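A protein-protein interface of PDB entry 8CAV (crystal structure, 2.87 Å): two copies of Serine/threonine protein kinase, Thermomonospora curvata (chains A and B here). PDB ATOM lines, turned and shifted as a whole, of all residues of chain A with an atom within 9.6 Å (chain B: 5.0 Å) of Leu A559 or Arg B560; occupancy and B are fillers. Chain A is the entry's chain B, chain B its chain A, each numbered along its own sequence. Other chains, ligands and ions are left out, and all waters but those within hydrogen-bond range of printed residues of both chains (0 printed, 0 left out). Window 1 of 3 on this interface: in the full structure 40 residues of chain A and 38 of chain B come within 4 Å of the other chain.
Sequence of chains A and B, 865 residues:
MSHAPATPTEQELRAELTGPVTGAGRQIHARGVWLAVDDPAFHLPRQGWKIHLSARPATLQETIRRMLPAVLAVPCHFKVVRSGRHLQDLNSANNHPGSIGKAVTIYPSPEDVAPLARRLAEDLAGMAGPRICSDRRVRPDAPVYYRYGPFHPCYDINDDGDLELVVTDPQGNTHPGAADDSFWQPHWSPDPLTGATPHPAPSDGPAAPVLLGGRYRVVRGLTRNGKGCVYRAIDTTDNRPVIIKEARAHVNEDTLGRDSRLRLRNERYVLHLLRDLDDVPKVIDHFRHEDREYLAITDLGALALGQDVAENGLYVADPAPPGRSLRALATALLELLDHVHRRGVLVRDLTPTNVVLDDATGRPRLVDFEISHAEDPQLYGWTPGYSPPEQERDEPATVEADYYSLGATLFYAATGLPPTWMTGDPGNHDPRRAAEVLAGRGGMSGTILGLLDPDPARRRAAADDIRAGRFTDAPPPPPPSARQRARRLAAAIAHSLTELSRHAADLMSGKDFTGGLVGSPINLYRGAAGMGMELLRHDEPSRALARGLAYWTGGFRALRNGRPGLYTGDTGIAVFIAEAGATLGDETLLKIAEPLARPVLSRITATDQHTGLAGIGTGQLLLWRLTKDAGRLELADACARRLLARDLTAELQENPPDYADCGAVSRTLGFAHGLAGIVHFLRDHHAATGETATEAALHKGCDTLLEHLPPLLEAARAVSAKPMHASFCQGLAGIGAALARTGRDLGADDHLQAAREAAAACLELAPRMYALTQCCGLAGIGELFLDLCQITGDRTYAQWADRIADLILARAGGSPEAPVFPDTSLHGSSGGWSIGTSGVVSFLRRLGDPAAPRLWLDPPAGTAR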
ATOM      1  N   ARG A  46      45.898 -27.042 -21.165  1.00  0.00           N
ATOM      2  CA  ARG A  46      44.568 -27.557 -20.836  1.00  0.00           C
ATOM      3  C   ARG A  46      44.602 -28.892 -20.103  1.00  0.00           C
ATOM      4  O   ARG A  46      43.595 -29.280 -19.499  1.00  0.00           O
ATOM      5  CB  ARG A  46      43.732 -27.692 -22.114  1.00  0.00           C
ATOM      6  CG  ARG A  46      42.229 -27.552 -21.904  1.00  0.00           C
ATOM      7  CD  ARG A  46      41.759 -26.095 -21.881  1.00  0.00           C
ATOM      8  NE  ARG A  46      42.127 -25.336 -23.075  1.00  0.00           N
ATOM      9  CZ  ARG A  46      41.628 -25.539 -24.288  1.00  0.00           C
ATOM     10  NH1 ARG A  46      40.804 -26.544 -24.538  1.00  0.00           N
ATOM     11  NH2 ARG A  46      41.968 -24.715 -25.274  1.00  0.00           N
ATOM     12  N   HIS A 152      41.575 -27.788 -17.218  1.00  0.00           N
ATOM     13  CA  HIS A 152      40.299 -27.126 -17.407  1.00  0.00           C
ATOM     14  C   HIS A 152      39.196 -28.156 -17.622  1.00  0.00           C
ATOM     15  O   HIS A 152      39.406 -29.152 -18.323  1.00  0.00           O
ATOM     16  CB  HIS A 152      40.339 -26.177 -18.610  1.00  0.00           C
ATOM     17  CG  HIS A 152      41.464 -25.191 -18.566  1.00  0.00           C
ATOM     18  ND1 HIS A 152      42.762 -25.533 -18.875  1.00  0.00           N
ATOM     19  CD2 HIS A 152      41.488 -23.874 -18.254  1.00  0.00           C
ATOM     20  CE1 HIS A 152      43.534 -24.468 -18.766  1.00  0.00           C
ATOM     21  NE2 HIS A 152      42.786 -23.449 -18.384  1.00  0.00           N
ATOM     22  N   PRO A 153      38.026 -27.966 -17.011  1.00  0.00           N
ATOM     23  CA  PRO A 153      36.897 -28.861 -17.290  1.00  0.00           C
ATOM     24  C   PRO A 153      36.521 -29.033 -18.756  1.00  0.00           C
ATOM     25  O   PRO A 153      35.644 -28.332 -19.272  1.00  0.00           O
ATOM     26  CB  PRO A 153      35.742 -28.208 -16.508  1.00  0.00           C
ATOM     27  CG  PRO A 153      36.384 -27.159 -15.594  1.00  0.00           C
ATOM     28  CD  PRO A 153      37.867 -27.326 -15.695  1.00  0.00           C
ATOM     29  N   CYS A 154      37.164 -29.983 -19.432  1.00  0.00           N
ATOM     30  CA  CYS A 154      36.665 -30.507 -20.697  1.00  0.00           C
ATOM     31  C   CYS A 154      35.783 -31.714 -20.395  1.00  0.00           C
ATOM     32  O   CYS A 154      36.199 -32.618 -19.665  1.00  0.00           O
ATOM     33  CB  CYS A 154      37.809 -30.907 -21.625  1.00  0.00           C
ATOM     34  SG  CYS A 154      37.268 -31.450 -23.270  1.00  0.00           S
ATOM     35  N   TYR A 155      34.573 -31.726 -20.950  1.00  0.00           N
ATOM     36  CA  TYR A 155      33.613 -32.793 -20.704  1.00  0.00           C
ATOM     37  C   TYR A 155      33.228 -33.466 -22.011  1.00  0.00           C
ATOM     38  O   TYR A 155      32.856 -32.790 -22.976  1.00  0.00           O
ATOM     39  CB  TYR A 155      32.353 -32.260 -20.015  1.00  0.00           C
ATOM     40  CG  TYR A 155      32.555 -31.971 -18.553  1.00  0.00           C
ATOM     41  CD1 TYR A 155      32.664 -33.005 -17.637  1.00  0.00           C
ATOM     42  CD2 TYR A 155      32.644 -30.664 -18.085  1.00  0.00           C
ATOM     43  CE1 TYR A 155      32.854 -32.754 -16.299  1.00  0.00           C
ATOM     44  CE2 TYR A 155      32.834 -30.403 -16.743  1.00  0.00           C
ATOM     45  CZ  TYR A 155      32.939 -31.454 -15.856  1.00  0.00           C
ATOM     46  OH  TYR A 155      33.129 -31.212 -14.516  1.00  0.00           O
ATOM     47  N   ASP A 156      33.302 -34.793 -22.032  1.00  0.00           N
ATOM     48  CA  ASP A 156      32.813 -35.569 -23.161  1.00  0.00           C
ATOM     49  C   ASP A 156      31.685 -36.479 -22.696  1.00  0.00           C
ATOM     50  O   ASP A 156      31.520 -36.739 -21.498  1.00  0.00           O
ATOM     51  CB  ASP A 156      33.930 -36.396 -23.811  1.00  0.00           C
ATOM     52  CG  ASP A 156      33.567 -36.870 -25.211  1.00  0.00           C
ATOM     53  OD1 ASP A 156      32.451 -36.558 -25.679  1.00  0.00           O
ATOM     54  OD2 ASP A 156      34.400 -37.552 -25.845  1.00  0.00           O
ATOM     55  N   LEU A 163      28.114 -36.936 -18.777  1.00  0.00           N
ATOM     56  CA  LEU A 163      29.306 -36.177 -19.132  1.00  0.00           C
ATOM     57  C   LEU A 163      30.392 -36.428 -18.097  1.00  0.00           C
ATOM     58  O   LEU A 163      30.126 -36.399 -16.890  1.00  0.00           O
ATOM     59  CB  LEU A 163      29.008 -34.684 -19.230  1.00  0.00           C
ATOM     60  CG  LEU A 163      28.098 -34.254 -20.381  1.00  0.00           C
ATOM     61  CD1 LEU A 163      28.069 -32.734 -20.492  1.00  0.00           C
ATOM     62  CD2 LEU A 163      28.539 -34.888 -21.692  1.00  0.00           C
ATOM     63  N   PHE A 513      26.893 -28.692 -12.506  1.00  0.00           N
ATOM     64  CA  PHE A 513      27.829 -29.163 -13.521  1.00  0.00           C
ATOM     65  C   PHE A 513      29.212 -29.475 -12.956  1.00  0.00           C
ATOM     66  O   PHE A 513      30.009 -30.118 -13.646  1.00  0.00           O
ATOM     67  CB  PHE A 513      27.965 -28.136 -14.649  1.00  0.00           C
ATOM     68  CG  PHE A 513      26.714 -27.963 -15.472  1.00  0.00           C
ATOM     69  CD1 PHE A 513      25.629 -28.810 -15.312  1.00  0.00           C
ATOM     70  CD2 PHE A 513      26.631 -26.952 -16.413  1.00  0.00           C
ATOM     71  CE1 PHE A 513      24.488 -28.647 -16.068  1.00  0.00           C
ATOM     72  CE2 PHE A 513      25.491 -26.786 -17.175  1.00  0.00           C
ATOM     73  CZ  PHE A 513      24.418 -27.633 -17.000  1.00  0.00           C
ATOM     74  N   TRP A 552      16.644 -24.126 -24.254  1.00  0.00           N
ATOM     75  CA  TRP A 552      17.923 -24.376 -23.602  1.00  0.00           C
ATOM     76  C   TRP A 552      18.554 -25.667 -24.103  1.00  0.00           C
ATOM     77  O   TRP A 552      19.771 -25.729 -24.311  1.00  0.00           O
ATOM     78  CB  TRP A 552      17.716 -24.438 -22.089  1.00  0.00           C
ATOM     79  CG  TRP A 552      18.969 -24.450 -21.268  1.00  0.00           C
ATOM     80  CD1 TRP A 552      19.578 -23.374 -20.695  1.00  0.00           C
ATOM     81  CD2 TRP A 552      19.753 -25.595 -20.903  1.00  0.00           C
ATOM     82  NE1 TRP A 552      20.692 -23.772 -20.000  1.00  0.00           N
ATOM     83  CE2 TRP A 552      20.824 -25.131 -20.114  1.00  0.00           C
ATOM     84  CE3 TRP A 552      19.656 -26.964 -21.171  1.00  0.00           C
ATOM     85  CZ2 TRP A 552      21.794 -25.986 -19.593  1.00  0.00           C
ATOM     86  CZ3 TRP A 552      20.620 -27.812 -20.650  1.00  0.00           C
ATOM     87  CH2 TRP A 552      21.673 -27.319 -19.871  1.00  0.00           C
ATOM     88  N   THR A 553      17.747 -26.714 -24.278  1.00  0.00           N
ATOM     89  CA  THR A 553      18.259 -27.983 -24.781  1.00  0.00           C
ATOM     90  C   THR A 553      18.741 -27.836 -26.218  1.00  0.00           C
ATOM     91  O   THR A 553      19.819 -28.324 -26.576  1.00  0.00           O
ATOM     92  CB  THR A 553      17.178 -29.062 -24.692  1.00  0.00           C
ATOM     93  OG1 THR A 553      16.900 -29.361 -23.317  1.00  0.00           O
ATOM     94  CG2 THR A 553      17.622 -30.330 -25.409  1.00  0.00           C
ATOM     95  N   GLY A 554      17.944 -27.182 -27.060  1.00  0.00           N
ATOM     96  CA  GLY A 554      18.386 -26.929 -28.419  1.00  0.00           C
ATOM     97  C   GLY A 554      19.732 -26.241 -28.457  1.00  0.00           C
ATOM     98  O   GLY A 554      20.590 -26.570 -29.280  1.00  0.00           O
ATOM     99  N   GLY A 555      19.944 -25.286 -27.549  1.00  0.00           N
ATOM    100  CA  GLY A 555      21.219 -24.586 -27.513  1.00  0.00           C
ATOM    101  C   GLY A 555      22.353 -25.455 -26.999  1.00  0.00           C
ATOM    102  O   GLY A 555      23.414 -25.547 -27.624  1.00  0.00           O
ATOM    103  N   PHE A 556      22.150 -26.094 -25.842  1.00  0.00           N
ATOM    104  CA  PHE A 556      23.183 -26.960 -25.283  1.00  0.00           C
ATOM    105  C   PHE A 556      23.600 -28.034 -26.277  1.00  0.00           C
ATOM    106  O   PHE A 556      24.767 -28.435 -26.305  1.00  0.00           O
ATOM    107  CB  PHE A 556      22.699 -27.621 -23.986  1.00  0.00           C
ATOM    108  CG  PHE A 556      23.785 -28.363 -23.239  1.00  0.00           C
ATOM    109  CD1 PHE A 556      24.199 -29.622 -23.647  1.00  0.00           C
ATOM    110  CD2 PHE A 556      24.394 -27.796 -22.131  1.00  0.00           C
ATOM    111  CE1 PHE A 556      25.202 -30.298 -22.968  1.00  0.00           C
ATOM    112  CE2 PHE A 556      25.395 -28.466 -21.445  1.00  0.00           C
ATOM    113  CZ  PHE A 556      25.799 -29.718 -21.868  1.00  0.00           C
ATOM    114  N   ARG A 557      22.664 -28.507 -27.102  1.00  0.00           N
ATOM    115  CA  ARG A 557      22.952 -29.645 -27.968  1.00  0.00           C
ATOM    116  C   ARG A 557      23.860 -29.261 -29.131  1.00  0.00           C
ATOM    117  O   ARG A 557      24.598 -30.111 -29.640  1.00  0.00           O
ATOM    118  CB  ARG A 557      21.643 -30.244 -28.485  1.00  0.00           C
ATOM    119  CG  ARG A 557      21.818 -31.468 -29.377  1.00  0.00           C
ATOM    120  CD  ARG A 557      22.452 -32.619 -28.609  1.00  0.00           C
ATOM    121  NE  ARG A 557      22.982 -33.666 -29.477  1.00  0.00           N
ATOM    122  CZ  ARG A 557      24.045 -33.526 -30.258  1.00  0.00           C
ATOM    123  NH1 ARG A 557      24.653 -32.359 -30.397  1.00  0.00           N
ATOM    124  NH2 ARG A 557      24.511 -34.583 -30.916  1.00  0.00           N
ATOM    125  N   ALA A 558      23.835 -27.997 -29.548  1.00  0.00           N
ATOM    126  CA  ALA A 558      24.573 -27.583 -30.734  1.00  0.00           C
ATOM    127  C   ALA A 558      26.080 -27.694 -30.529  1.00  0.00           C
ATOM    128  O   ALA A 558      26.619 -27.247 -29.511  1.00  0.00           O
ATOM    129  CB  ALA A 558      24.198 -26.148 -31.109  1.00  0.00           C
ATOM    130  N   LEU A 559      26.749 -28.308 -31.506  1.00  0.00           N
ATOM    131  CA  LEU A 559      28.210 -28.339 -31.605  1.00  0.00           C
ATOM    132  C   LEU A 559      28.868 -28.961 -30.372  1.00  0.00           C
ATOM    133  O   LEU A 559      29.852 -28.446 -29.837  1.00  0.00           O
ATOM    134  CB  LEU A 559      28.772 -26.938 -31.863  1.00  0.00           C
ATOM    135  CG  LEU A 559      28.486 -26.300 -33.223  1.00  0.00           C
ATOM    136  CD1 LEU A 559      29.164 -24.938 -33.305  1.00  0.00           C
ATOM    137  CD2 LEU A 559      28.940 -27.186 -34.370  1.00  0.00           C
ATOM    138  N   ARG A 560      28.327 -30.097 -29.933  1.00  0.00           N
ATOM    139  CA  ARG A 560      29.042 -30.955 -28.998  1.00  0.00           C
ATOM    140  C   ARG A 560      28.683 -32.406 -29.289  1.00  0.00           C
ATOM    141  O   ARG A 560      27.732 -32.702 -30.016  1.00  0.00           O
ATOM    142  CB  ARG A 560      28.741 -30.604 -27.533  1.00  0.00           C
ATOM    143  CG  ARG A 560      27.273 -30.477 -27.185  1.00  0.00           C
ATOM    144  CD  ARG A 560      27.060 -30.339 -25.676  1.00  0.00           C
ATOM    145  NE  ARG A 560      28.052 -29.494 -25.014  1.00  0.00           N
ATOM    146  CZ  ARG A 560      27.918 -28.190 -24.796  1.00  0.00           C
ATOM    147  NH1 ARG A 560      26.868 -27.516 -25.237  1.00  0.00           N
ATOM    148  NH2 ARG A 560      28.864 -27.547 -24.115  1.00  0.00           N
ATOM    149  N   ASN A 561      29.475 -33.311 -28.714  1.00  0.00           N
ATOM    150  CA  ASN A 561      29.240 -34.739 -28.874  1.00  0.00           C
ATOM    151  C   ASN A 561      27.815 -35.100 -28.474  1.00  0.00           C
ATOM    152  O   ASN A 561      27.194 -34.443 -27.631  1.00  0.00           O
ATOM    153  CB  ASN A 561      30.231 -35.536 -28.023  1.00  0.00           C
ATOM    154  CG  ASN A 561      31.385 -36.089 -28.833  1.00  0.00           C
ATOM    155  OD1 ASN A 561      32.298 -35.359 -29.220  1.00  0.00           O
ATOM    156  ND2 ASN A 561      31.356 -37.394 -29.081  1.00  0.00           N
ATOM    157  N   GLY A 562      27.294 -36.161 -29.091  1.00  0.00           N
ATOM    158  CA  GLY A 562      26.006 -36.707 -28.727  1.00  0.00           C
ATOM    159  C   GLY A 562      26.037 -38.224 -28.740  1.00  0.00           C
ATOM    160  O   GLY A 562      27.073 -38.840 -28.997  1.00  0.00           O
ATOM    161  N   LEU A 596      17.444 -32.920 -35.734  1.00  0.00           N
ATOM    162  CA  LEU A 596      18.181 -33.427 -34.581  1.00  0.00           C
ATOM    163  C   LEU A 596      18.564 -34.900 -34.726  1.00  0.00           C
ATOM    164  O   LEU A 596      19.714 -35.197 -35.065  1.00  0.00           O
ATOM    165  CB  LEU A 596      17.367 -33.174 -33.306  1.00  0.00           C
ATOM    166  CG  LEU A 596      17.962 -32.187 -32.287  1.00  0.00           C
ATOM    167  CD1 LEU A 596      18.873 -31.142 -32.918  1.00  0.00           C
ATOM    168  CD2 LEU A 596      16.866 -31.462 -31.505  1.00  0.00           C
ATOM    169  N   TYR B 155      35.225 -27.400 -32.665  1.00  0.00           N
ATOM    170  CA  TYR B 155      35.369 -25.952 -32.714  1.00  0.00           C
ATOM    171  C   TYR B 155      35.848 -25.415 -31.370  1.00  0.00           C
ATOM    172  O   TYR B 155      35.408 -25.877 -30.314  1.00  0.00           O
ATOM    173  CB  TYR B 155      34.039 -25.280 -33.089  1.00  0.00           C
ATOM    174  CG  TYR B 155      33.537 -25.581 -34.488  1.00  0.00           C
ATOM    175  CD1 TYR B 155      33.885 -24.768 -35.561  1.00  0.00           C
ATOM    176  CD2 TYR B 155      32.704 -26.664 -34.733  1.00  0.00           C
ATOM    177  CE1 TYR B 155      33.422 -25.034 -36.839  1.00  0.00           C
ATOM    178  CE2 TYR B 155      32.238 -26.936 -36.006  1.00  0.00           C
ATOM    179  CZ  TYR B 155      32.603 -26.118 -37.054  1.00  0.00           C
ATOM    180  OH  TYR B 155      32.142 -26.386 -38.323  1.00  0.00           O
ATOM    181  N   LEU B 163      33.720 -19.147 -33.906  1.00  0.00           N
ATOM    182  CA  LEU B 163      34.033 -20.546 -33.656  1.00  0.00           C
ATOM    183  C   LEU B 163      34.887 -21.098 -34.791  1.00  0.00           C
ATOM    184  O   LEU B 163      34.549 -20.925 -35.965  1.00  0.00           O
ATOM    185  CB  LEU B 163      32.741 -21.354 -33.511  1.00  0.00           C
ATOM    186  CG  LEU B 163      31.922 -21.002 -32.267  1.00  0.00           C
ATOM    187  CD1 LEU B 163      30.638 -21.818 -32.201  1.00  0.00           C
ATOM    188  CD2 LEU B 163      32.752 -21.205 -31.004  1.00  0.00           C
ATOM    189  N   PHE B 513      26.023 -23.360 -38.855  1.00  0.00           N
ATOM    190  CA  PHE B 513      27.148 -24.120 -38.328  1.00  0.00           C
ATOM    191  C   PHE B 513      27.749 -25.011 -39.405  1.00  0.00           C
ATOM    192  O   PHE B 513      28.820 -25.591 -39.190  1.00  0.00           O
ATOM    193  CB  PHE B 513      26.741 -24.987 -37.130  1.00  0.00           C
ATOM    194  CG  PHE B 513      25.975 -24.255 -36.044  1.00  0.00           C
ATOM    195  CD1 PHE B 513      25.691 -22.899 -36.130  1.00  0.00           C
ATOM    196  CD2 PHE B 513      25.540 -24.944 -34.927  1.00  0.00           C
ATOM    197  CE1 PHE B 513      24.980 -22.258 -35.136  1.00  0.00           C
ATOM    198  CE2 PHE B 513      24.836 -24.305 -33.927  1.00  0.00           C
ATOM    199  CZ  PHE B 513      24.558 -22.961 -34.032  1.00  0.00           C
ATOM    200  N   PHE B 556      23.407 -22.989 -24.714  1.00  0.00           N
ATOM    201  CA  PHE B 556      24.556 -23.110 -25.602  1.00  0.00           C
ATOM    202  C   PHE B 556      25.844 -22.734 -24.882  1.00  0.00           C
ATOM    203  O   PHE B 556      26.887 -23.365 -25.091  1.00  0.00           O
ATOM    204  CB  PHE B 556      24.367 -22.226 -26.835  1.00  0.00           C
ATOM    205  CG  PHE B 556      25.518 -22.288 -27.800  1.00  0.00           C
ATOM    206  CD1 PHE B 556      26.717 -21.649 -27.516  1.00  0.00           C
ATOM    207  CD2 PHE B 556      25.403 -22.989 -28.990  1.00  0.00           C
ATOM    208  CE1 PHE B 556      27.779 -21.710 -28.391  1.00  0.00           C
ATOM    209  CE2 PHE B 556      26.463 -23.050 -29.877  1.00  0.00           C
ATOM    210  CZ  PHE B 556      27.655 -22.411 -29.576  1.00  0.00           C
ATOM    211  N   ARG B 557      25.798 -21.691 -24.053  1.00  0.00           N
ATOM    212  CA  ARG B 557      26.993 -21.243 -23.351  1.00  0.00           C
ATOM    213  C   ARG B 557      27.493 -22.282 -22.359  1.00  0.00           C
ATOM    214  O   ARG B 557      28.687 -22.291 -22.039  1.00  0.00           O
ATOM    215  CB  ARG B 557      26.701 -19.918 -22.637  1.00  0.00           C
ATOM    216  CG  ARG B 557      27.873 -19.326 -21.859  1.00  0.00           C
ATOM    217  CD  ARG B 557      28.968 -18.819 -22.780  1.00  0.00           C
ATOM    218  NE  ARG B 557      30.218 -18.595 -22.062  1.00  0.00           N
ATOM    219  CZ  ARG B 557      31.029 -19.562 -21.656  1.00  0.00           C
ATOM    220  NH1 ARG B 557      30.729 -20.838 -21.840  1.00  0.00           N
ATOM    221  NH2 ARG B 557      32.168 -19.242 -21.049  1.00  0.00           N
ATOM    222  N   ALA B 558      26.616 -23.168 -21.897  1.00  0.00           N
ATOM    223  CA  ALA B 558      26.957 -24.086 -20.820  1.00  0.00           C
ATOM    224  C   ALA B 558      28.083 -25.031 -21.221  1.00  0.00           C
ATOM    225  O   ALA B 558      28.054 -25.642 -22.293  1.00  0.00           O
ATOM    226  CB  ALA B 558      25.719 -24.889 -20.414  1.00  0.00           C
ATOM    227  N   LEU B 559      29.081 -25.139 -20.342  1.00  0.00           N
ATOM    228  CA  LEU B 559      30.138 -26.144 -20.442  1.00  0.00           C
ATOM    229  C   LEU B 559      30.885 -26.079 -21.773  1.00  0.00           C
ATOM    230  O   LEU B 559      31.200 -27.108 -22.375  1.00  0.00           O
ATOM    231  CB  LEU B 559      29.580 -27.552 -20.215  1.00  0.00           C
ATOM    232  CG  LEU B 559      29.050 -27.892 -18.819  1.00  0.00           C
ATOM    233  CD1 LEU B 559      28.703 -29.372 -18.731  1.00  0.00           C
ATOM    234  CD2 LEU B 559      30.053 -27.521 -17.742  1.00  0.00           C
ATOM    235  N   ARG B 560      31.190 -24.870 -22.238  1.00  0.00           N
ATOM    236  CA  ARG B 560      32.138 -24.710 -23.331  1.00  0.00           C
ATOM    237  C   ARG B 560      33.008 -23.485 -23.088  1.00  0.00           C
ATOM    238  O   ARG B 560      32.664 -22.585 -22.318  1.00  0.00           O
ATOM    239  CB  ARG B 560      31.457 -24.611 -24.707  1.00  0.00           C
ATOM    240  CG  ARG B 560      30.332 -23.604 -24.811  1.00  0.00           C
ATOM    241  CD  ARG B 560      29.928 -23.372 -26.271  1.00  0.00           C
ATOM    242  NE  ARG B 560      29.989 -24.577 -27.094  1.00  0.00           N
ATOM    243  CZ  ARG B 560      28.962 -25.381 -27.342  1.00  0.00           C
ATOM    244  NH1 ARG B 560      27.773 -25.176 -26.798  1.00  0.00           N
ATOM    245  NH2 ARG B 560      29.131 -26.413 -28.164  1.00  0.00           N
ATOM    246  N   ASN B 561      34.155 -23.480 -23.759  1.00  0.00           N
ATOM    247  CA  ASN B 561      35.133 -22.407 -23.638  1.00  0.00           C
ATOM    248  C   ASN B 561      34.613 -21.134 -24.297  1.00  0.00           C
ATOM    249  O   ASN B 561      33.865 -21.182 -25.276  1.00  0.00           O
ATOM    250  CB  ASN B 561      36.448 -22.855 -24.282  1.00  0.00           C
ATOM    251  CG  ASN B 561      37.478 -21.751 -24.357  1.00  0.00           C
ATOM    252  OD1 ASN B 561      37.627 -20.955 -23.432  1.00  0.00           O
ATOM    253  ND2 ASN B 561      38.204 -21.702 -25.469  1.00  0.00           N
ATOM    254  N   GLY B 562      35.020 -19.986 -23.753  1.00  0.00           N
ATOM    255  CA  GLY B 562      34.529 -18.710 -24.230  1.00  0.00           C
ATOM    256  C   GLY B 562      35.508 -17.585 -23.971  1.00  0.00           C
ATOM    257  O   GLY B 562      36.617 -17.799 -23.481  1.00  0.00           O
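Among the printed residues, pairs that only touch across the chains: Gly A555 with Phe B556, Ala A558 with Phe B513, Phe A556 with Phe B556, Phe A513 with Leu B559, Leu A559 with Leu B163, Phe A556 with Ala B558, Leu A559 with Phe B513, Leu A559 with Tyr B155, Phe A513 with Ala B558, Leu A163 with Leu B559 and Ala A558 with Phe B556.
Of the 10 printed residues of chain B, 7 touch a printed residue of chain A. Hydrophobic or aromatic side chains of chain B that line the printed part of chain A: Tyr B155, Leu B163, Phe B513, Phe B556, Ala B558 and Leu B559. Hydrophobic or aromatic side chains of chain A within 4 Å of the printed part of chain B: Leu A163, Phe A513, Phe A556, Ala A558 and Leu A559. Among the printed residues, no Asp or Glu carboxylate lies within 4 Å of a Lys or Arg side-chain nitrogen of the other chain.
Leu A559 touches four residues of chain B. Of chain A, only Ala A558 (3.0 Å), Leu A559 (2.7 Å) and Arg A560 (3.0 Å) come within 4 Å of Arg B560. Of the printed residues of chain A, Leu B559 touches Leu A163 (3.8 Å), Phe A513 (3.5 Å) and Arg A560 (2.9 Å). Of the printed residues of chain A, Tyr B155 touches Leu A559. Of the printed residues of chain A, Leu B163 touches Leu A559. Printed residues of chain B within 4 Å of Phe A513: Ala B558 and Leu B559. The nearest residue of chain B that does not touch Leu A559 is Phe B556 (4.8 Å). The nearest printed residue of chain A that does not touch Arg B560 is Gly A555 (4.5 Å).
Phe A513 touches Ala B558, and with the chains exchanged Ala A558 touches Phe B513. Phe A513 touches Leu B559, and with the chains exchanged Leu A559 touches Phe B513. Phe B556 touches its own counterpart, Phe A556. Phe A556 touches Ala B558, and with the chains exchanged Ala A558 touches Phe B556. 10 positions are printed for both chains. Of the 16 pairs that touch across the chains among the printed residues, 14 have their exchanged pair printed and touching as well.
The backbone carbonyl oxygen of Ala B558 sits at hydrogen-bond distance from the guanidinium group of Arg A560 (2.8 Å). O of Leu B559 lies within hydrogen-bond range of NH2 of Arg A560 (2.9 Å). NH2 of Arg B560 lies within hydrogen-bond range of O of Ala A558 (3.0 Å). The guanidinium group (NH2) of Arg B560 sits at hydrogen-bond distance from the backbone carbonyl oxygen (O) of Leu A559, 2.7 Å away. NH1 of Arg A560 sits close to NH1 of Arg B560 (3.0 Å).
The guanidinium group (NH1) of Arg B560 is in hydrogen-bond range of the backbone carbonyl oxygen (O) of Phe B556 (2.6 Å). The backbone carbonyl oxygen (O) of Arg B560 sits at hydrogen-bond distance from the guanidinium group (NH1) of Arg B557, 2.7 Å away. The side-chain hydroxyl of Tyr A155 lies within hydrogen-bond range of the backbone carbonyl oxygen of Phe A513 (3.4 Å). The backbone carbonyl oxygen (O) of Phe A556 is in hydrogen-bond range of the guanidinium group (NH1) of Arg A560, 2.5 Å away. NH1 of Arg A557 sits at hydrogen-bond distance from O of Arg A560, 3.1 Å away.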
